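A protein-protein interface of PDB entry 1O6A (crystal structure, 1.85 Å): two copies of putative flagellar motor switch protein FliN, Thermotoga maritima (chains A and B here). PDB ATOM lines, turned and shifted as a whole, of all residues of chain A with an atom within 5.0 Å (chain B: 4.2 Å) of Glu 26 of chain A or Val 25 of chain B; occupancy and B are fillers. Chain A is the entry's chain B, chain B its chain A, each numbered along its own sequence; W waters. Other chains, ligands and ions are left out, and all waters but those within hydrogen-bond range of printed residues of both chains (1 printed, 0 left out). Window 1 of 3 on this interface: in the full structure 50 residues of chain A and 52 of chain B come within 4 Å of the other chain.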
ATOM      1  N   THR A  24     -19.849  30.988 -25.202  1.00  0.00           N
ATOM      2  CA  THR A  24     -18.823  30.062 -24.690  1.00  0.00           C
ATOM      3  C   THR A  24     -18.143  29.395 -25.859  1.00  0.00           C
ATOM      4  O   THR A  24     -18.791  29.061 -26.863  1.00  0.00           O
ATOM      5  CB  THR A  24     -19.478  29.007 -23.804  1.00  0.00           C
ATOM      6  OG1 THR A  24     -19.987  29.618 -22.625  1.00  0.00           O
ATOM      7  CG2 THR A  24     -18.426  28.019 -23.266  1.00  0.00           C
ATOM      8  N   VAL A  25     -16.821  29.246 -25.792  1.00  0.00           N
ATOM      9  CA  VAL A  25     -16.083  28.508 -26.786  1.00  0.00           C
ATOM     10  C   VAL A  25     -15.582  27.240 -26.111  1.00  0.00           C
ATOM     11  O   VAL A  25     -14.882  27.298 -25.079  1.00  0.00           O
ATOM     12  CB  VAL A  25     -14.934  29.334 -27.340  1.00  0.00           C
ATOM     13  CG1 VAL A  25     -14.085  28.524 -28.309  1.00  0.00           C
ATOM     14  CG2 VAL A  25     -15.509  30.564 -28.058  1.00  0.00           C
ATOM     15  N   GLU A  26     -15.978  26.098 -26.667  1.00  0.00           N
ATOM     16  CA  GLU A  26     -15.637  24.819 -26.120  1.00  0.00           C
ATOM     17  C   GLU A  26     -14.610  24.107 -27.003  1.00  0.00           C
ATOM     18  O   GLU A  26     -14.699  24.059 -28.209  1.00  0.00           O
ATOM     19  CB  GLU A  26     -16.853  23.931 -25.976  1.00  0.00           C
ATOM     20  CG  GLU A  26     -17.790  24.345 -24.870  1.00  0.00           C
ATOM     21  CD  GLU A  26     -18.929  23.345 -24.684  1.00  0.00           C
ATOM     22  OE1 GLU A  26     -18.900  22.252 -25.310  1.00  0.00           O
ATOM     23  OE2 GLU A  26     -19.836  23.646 -23.867  1.00  0.00           O
ATOM     24  N   LEU A  27     -13.627  23.537 -26.345  1.00  0.00           N
ATOM     25  CA  LEU A  27     -12.625  22.675 -26.961  1.00  0.00           C
ATOM     26  C   LEU A  27     -13.198  21.293 -27.221  1.00  0.00           C
ATOM     27  O   LEU A  27     -12.740  20.568 -28.085  1.00  0.00           O
ATOM     28  CB  LEU A  27     -11.419  22.526 -26.014  1.00  0.00           C
ATOM     29  CG  LEU A  27     -10.317  21.566 -26.478  1.00  0.00           C
ATOM     30  CD1 LEU A  27      -9.566  22.184 -27.664  1.00  0.00           C
ATOM     31  CD2 LEU A  27      -9.354  21.240 -25.338  1.00  0.00           C
ATOM     32  N   GLY A  28     -14.166  20.886 -26.403  1.00  0.00           N
ATOM     33  CA  GLY A  28     -14.749  19.574 -26.558  1.00  0.00           C
ATOM     34  C   GLY A  28     -15.451  19.113 -25.291  1.00  0.00           C
ATOM     35  O   GLY A  28     -15.399  19.789 -24.257  1.00  0.00           O
ATOM     36  N   ARG A  29     -16.044  17.929 -25.387  1.00  0.00           N
ATOM     37  CA  ARG A  29     -16.789  17.278 -24.309  1.00  0.00           C
ATOM     38  C   ARG A  29     -16.466  15.796 -24.197  1.00  0.00           C
ATOM     39  O   ARG A  29     -15.939  15.167 -25.128  1.00  0.00           O
ATOM     40  CB  ARG A  29     -18.289  17.411 -24.495  1.00  0.00           C
ATOM     41  CG  ARG A  29     -18.793  18.784 -24.609  1.00  0.00           C
ATOM     42  CD  ARG A  29     -20.329  18.847 -24.747  1.00  0.00           C
ATOM     43  NE  ARG A  29     -20.731  20.239 -24.697  1.00  0.00           N
ATOM     44  CZ  ARG A  29     -21.950  20.647 -24.467  1.00  0.00           C
ATOM     45  NH1 ARG A  29     -22.912  19.768 -24.249  1.00  0.00           N
ATOM     46  NH2 ARG A  29     -22.204  21.946 -24.443  1.00  0.00           N
ATOM     47  N   LEU A  48     -11.231  14.169 -25.222  1.00  0.00           N
ATOM     48  CA  LEU A  48     -12.500  14.766 -25.629  1.00  0.00           C
ATOM     49  C   LEU A  48     -12.985  14.229 -26.979  1.00  0.00           C
ATOM     50  O   LEU A  48     -12.245  13.611 -27.743  1.00  0.00           O
ATOM     51  CB  LEU A  48     -12.362  16.273 -25.696  1.00  0.00           C
ATOM     52  CG  LEU A  48     -11.797  16.894 -24.431  1.00  0.00           C
ATOM     53  CD1 LEU A  48     -11.470  18.393 -24.742  1.00  0.00           C
ATOM     54  CD2 LEU A  48     -12.758  16.740 -23.266  1.00  0.00           C
ATOM     55  N   LYS A  50     -13.762  15.846 -29.705  1.00  0.00           N
ATOM     56  CA  LYS A  50     -13.375  16.600 -30.880  1.00  0.00           C
ATOM     57  C   LYS A  50     -12.065  16.096 -31.494  1.00  0.00           C
ATOM     58  O   LYS A  50     -11.096  15.804 -30.814  1.00  0.00           O
ATOM     59  CB  LYS A  50     -13.241  18.088 -30.495  1.00  0.00           C
ATOM     60  CG  LYS A  50     -13.010  19.061 -31.703  1.00  0.00           C
ATOM     61  CD  LYS A  50     -13.082  20.568 -31.285  1.00  0.00           C
ATOM     62  CE  LYS A  50     -14.500  20.947 -30.850  1.00  0.00           C
ATOM     63  NZ  LYS A  50     -15.478  20.920 -31.998  1.00  0.00           N
ATOM     64  N   VAL A  56     -13.243  24.559 -33.215  1.00  0.00           N
ATOM     65  CA  VAL A  56     -13.831  24.559 -31.886  1.00  0.00           C
ATOM     66  C   VAL A  56     -15.246  25.132 -31.889  1.00  0.00           C
ATOM     67  O   VAL A  56     -15.614  25.871 -32.803  1.00  0.00           O
ATOM     68  CB  VAL A  56     -12.914  25.330 -30.878  1.00  0.00           C
ATOM     69  CG1 VAL A  56     -11.523  24.674 -30.814  1.00  0.00           C
ATOM     70  CG2 VAL A  56     -12.787  26.784 -31.210  1.00  0.00           C
ATOM     71  N   ASP A  57     -16.048  24.749 -30.886  1.00  0.00           N
ATOM     72  CA  ASP A  57     -17.484  25.090 -30.859  1.00  0.00           C
ATOM     73  C   ASP A  57     -17.749  26.438 -30.258  1.00  0.00           C
ATOM     74  O   ASP A  57     -17.165  26.774 -29.243  1.00  0.00           O
ATOM     75  CB  ASP A  57     -18.260  24.058 -30.040  1.00  0.00           C
ATOM     76  CG  ASP A  57     -18.112  22.636 -30.591  1.00  0.00           C
ATOM     77  OD1 ASP A  57     -18.027  22.476 -31.814  1.00  0.00           O
ATOM     78  OD2 ASP A  57     -18.027  21.640 -29.856  1.00  0.00           O
ATOM     79  N   LEU A  59     -20.839  28.528 -28.722  1.00  0.00           N
ATOM     80  CA  LEU A  59     -22.172  28.355 -28.242  1.00  0.00           C
ATOM     81  C   LEU A  59     -22.687  29.717 -27.761  1.00  0.00           C
ATOM     82  O   LEU A  59     -21.960  30.496 -27.135  1.00  0.00           O
ATOM     83  CB  LEU A  59     -22.222  27.329 -27.123  1.00  0.00           C
ATOM     84  CG  LEU A  59     -21.935  25.870 -27.533  1.00  0.00           C
ATOM     85  CD1 LEU A  59     -20.496  25.527 -27.329  1.00  0.00           C
ATOM     86  CD2 LEU A  59     -22.761  24.943 -26.689  1.00  0.00           C
ATOM     87  N   THR B  24     -17.096  19.250 -19.814  1.00  0.00           N
ATOM     88  CA  THR B  24     -16.924  20.264 -20.865  1.00  0.00           C
ATOM     89  C   THR B  24     -15.619  20.997 -20.612  1.00  0.00           C
ATOM     90  O   THR B  24     -15.279  21.279 -19.454  1.00  0.00           O
ATOM     91  CB  THR B  24     -18.112  21.276 -20.862  1.00  0.00           C
ATOM     92  OG1 THR B  24     -18.237  21.901 -19.575  1.00  0.00           O
ATOM     93  CG2 THR B  24     -19.455  20.611 -21.065  1.00  0.00           C
ATOM     94  N   VAL B  25     -14.885  21.320 -21.679  1.00  0.00           N
ATOM     95  CA  VAL B  25     -13.663  22.049 -21.564  1.00  0.00           C
ATOM     96  C   VAL B  25     -13.859  23.332 -22.369  1.00  0.00           C
ATOM     97  O   VAL B  25     -14.267  23.315 -23.552  1.00  0.00           O
ATOM     98  CB  VAL B  25     -12.506  21.248 -22.093  1.00  0.00           C
ATOM     99  CG1 VAL B  25     -11.222  22.063 -22.106  1.00  0.00           C
ATOM    100  CG2 VAL B  25     -12.326  19.936 -21.282  1.00  0.00           C
ATOM    101  N   GLU B  26     -13.630  24.453 -21.698  1.00  0.00           N
ATOM    102  CA  GLU B  26     -13.897  25.786 -22.262  1.00  0.00           C
ATOM    103  C   GLU B  26     -12.604  26.533 -22.480  1.00  0.00           C
ATOM    104  O   GLU B  26     -11.703  26.563 -21.633  1.00  0.00           O
ATOM    105  CB  GLU B  26     -14.741  26.624 -21.304  1.00  0.00           C
ATOM    106  CG  GLU B  26     -16.145  26.120 -21.099  1.00  0.00           C
ATOM    107  CD  GLU B  26     -17.011  27.058 -20.289  1.00  0.00           C
ATOM    108  OE1 GLU B  26     -16.562  28.178 -19.957  1.00  0.00           O
ATOM    109  OE2 GLU B  26     -18.174  26.681 -20.011  1.00  0.00           O
ATOM    110  N   VAL B  56      -7.052  26.209 -19.717  1.00  0.00           N
ATOM    111  CA  VAL B  56      -8.451  26.065 -20.126  1.00  0.00           C
ATOM    112  C   VAL B  56      -9.245  25.564 -18.939  1.00  0.00           C
ATOM    113  O   VAL B  56      -8.676  24.993 -17.989  1.00  0.00           O
ATOM    114  CB  VAL B  56      -8.645  25.111 -21.324  1.00  0.00           C
ATOM    115  CG1 VAL B  56      -7.918  25.683 -22.527  1.00  0.00           C
ATOM    116  CG2 VAL B  56      -8.230  23.704 -21.018  1.00  0.00           C
ATOM    117  N   ASP B  57     -10.529  25.820 -18.961  1.00  0.00           N
ATOM    118  CA  ASP B  57     -11.388  25.423 -17.857  1.00  0.00           C
ATOM    119  C   ASP B  57     -12.059  24.068 -18.074  1.00  0.00           C
ATOM    120  O   ASP B  57     -12.496  23.757 -19.180  1.00  0.00           O
ATOM    121  CB  ASP B  57     -12.477  26.457 -17.652  1.00  0.00           C
ATOM    122  CG  ASP B  57     -11.890  27.852 -17.460  1.00  0.00           C
ATOM    123  OD1 ASP B  57     -11.051  27.983 -16.542  1.00  0.00           O
ATOM    124  OD2 ASP B  57     -12.090  28.800 -18.252  1.00  0.00           O
ATOM    125  N   VAL B  79      -7.142  17.219 -22.555  1.00  0.00           N
ATOM    126  CA  VAL B  79      -6.628  18.187 -21.595  1.00  0.00           C
ATOM    127  C   VAL B  79      -5.850  17.426 -20.505  1.00  0.00           C
ATOM    128  O   VAL B  79      -6.275  16.350 -20.054  1.00  0.00           O
ATOM    129  CB  VAL B  79      -7.804  19.116 -21.082  1.00  0.00           C
ATOM    130  CG1 VAL B  79      -8.840  18.343 -20.252  1.00  0.00           C
ATOM    131  CG2 VAL B  79      -7.281  20.322 -20.315  1.00  0.00           C
HETATM  132  O   HOH W   1     -20.576  27.714 -20.728  1.00  0.00           O
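N of Leu 27 of chain A is in hydrogen-bond range of O of Val 25 of chain B, 2.9 Å away. O of Gly 28 of chain A is in hydrogen-bond range of N of Val 25 of chain B (3.0 Å).
The backbone NH (N) of Glu 26 of chain B lies within hydrogen-bond range of the backbone carbonyl oxygen (O) of Asp 57 of chain B. The backbone NH (N) of Leu 59 of chain A is in hydrogen-bond range of the backbone carbonyl oxygen (O) of Thr 24 of chain A (2.8 Å). NE of Arg 29 of chain A is in salt-bridge range of OE1 of Glu 26 of chain A (2.8 Å). N of Glu 26 of chain A lies within hydrogen-bond range of O of Asp 57 of chain A, 2.9 Å away.
Among the printed residues, pairs that only touch across the chains: Thr 24 of chain A with Glu 26 of chain B (3.4 Å), Val 25 of chain A with Glu 26 of chain B (3.3 Å), Glu 26 of chain A with Val 25 of chain B (3.3 Å), Gly 28 of chain A with Thr 24 of chain B (3.7 Å), Arg 29 of chain A with Thr 24 of chain B (3.9 Å) and Leu 48 of chain A with Val 25 of chain B (3.8 Å).
Of the printed residues of chain B, Thr 24 of chain A touches Glu 26. Of the printed residues of chain B, Glu 26 of chain A touches Val 25. Of the printed residues of chain B, Gly 28 of chain A touches Thr 24 and Val 25. Printed residues of chain B within 4 Å of Leu 48 of chain A: Val 25 (3.8 Å). Asp 57 of chain A touches none of the printed residues of chain B. Of the printed residues of chain A, Thr 24 of chain B touches Gly 28 (3.7 Å) and Arg 29 (3.9 Å). Of the printed residues of chain A, Val 25 of chain B touches Glu 26 (3.3 Å), Leu 27 (2.9 Å), Gly 28 (3.0 Å) and Leu 48 (3.8 Å). Of the printed residues of chain A, Glu 26 of chain B touches Thr 24 (3.4 Å) and Val 25 (3.3 Å). Val 56 of chain B touches none of the printed residues of chain A. The nearest printed residue of chain A that does not touch Val 25 of chain B is Val 25 of chain A (4.3 Å). The nearest printed residue of chain B that does not touch Leu 48 of chain A is Val 79 of chain B (5.0 Å).
Hydrophobic or aromatic side chains of chain A within 4 Å of the printed part of chain B: Leu 27 and Leu 48. Among the printed residues, 8 pairs touch across the chains. Among the printed residues, no Asp or Glu carboxylate lies within 4 Å of a Lys or Arg side-chain nitrogen of the other chain.
Thr 24 of chain A touches Glu 26 of chain B, but with the chains exchanged Glu 26 of chain A does not touch Thr 24 of chain B (4.1 Å). Val 25 of chain A touches Glu 26 of chain B, and with the chains exchanged Glu 26 of chain A touches Val 25 of chain B. Positions printed for both chains: 24, 25, 26, 56 and 57. Of the 8 pairs that touch across the chains among the printed residues, 2 have their exchanged pair printed and touching as well.
Water W1 lies within hydrogen-bond range of the side-chain carboxylate of Glu 26 of chain B (2.7 Å) and the side-chain hydroxyl of Thr 24 of chain A (2.8 Å).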
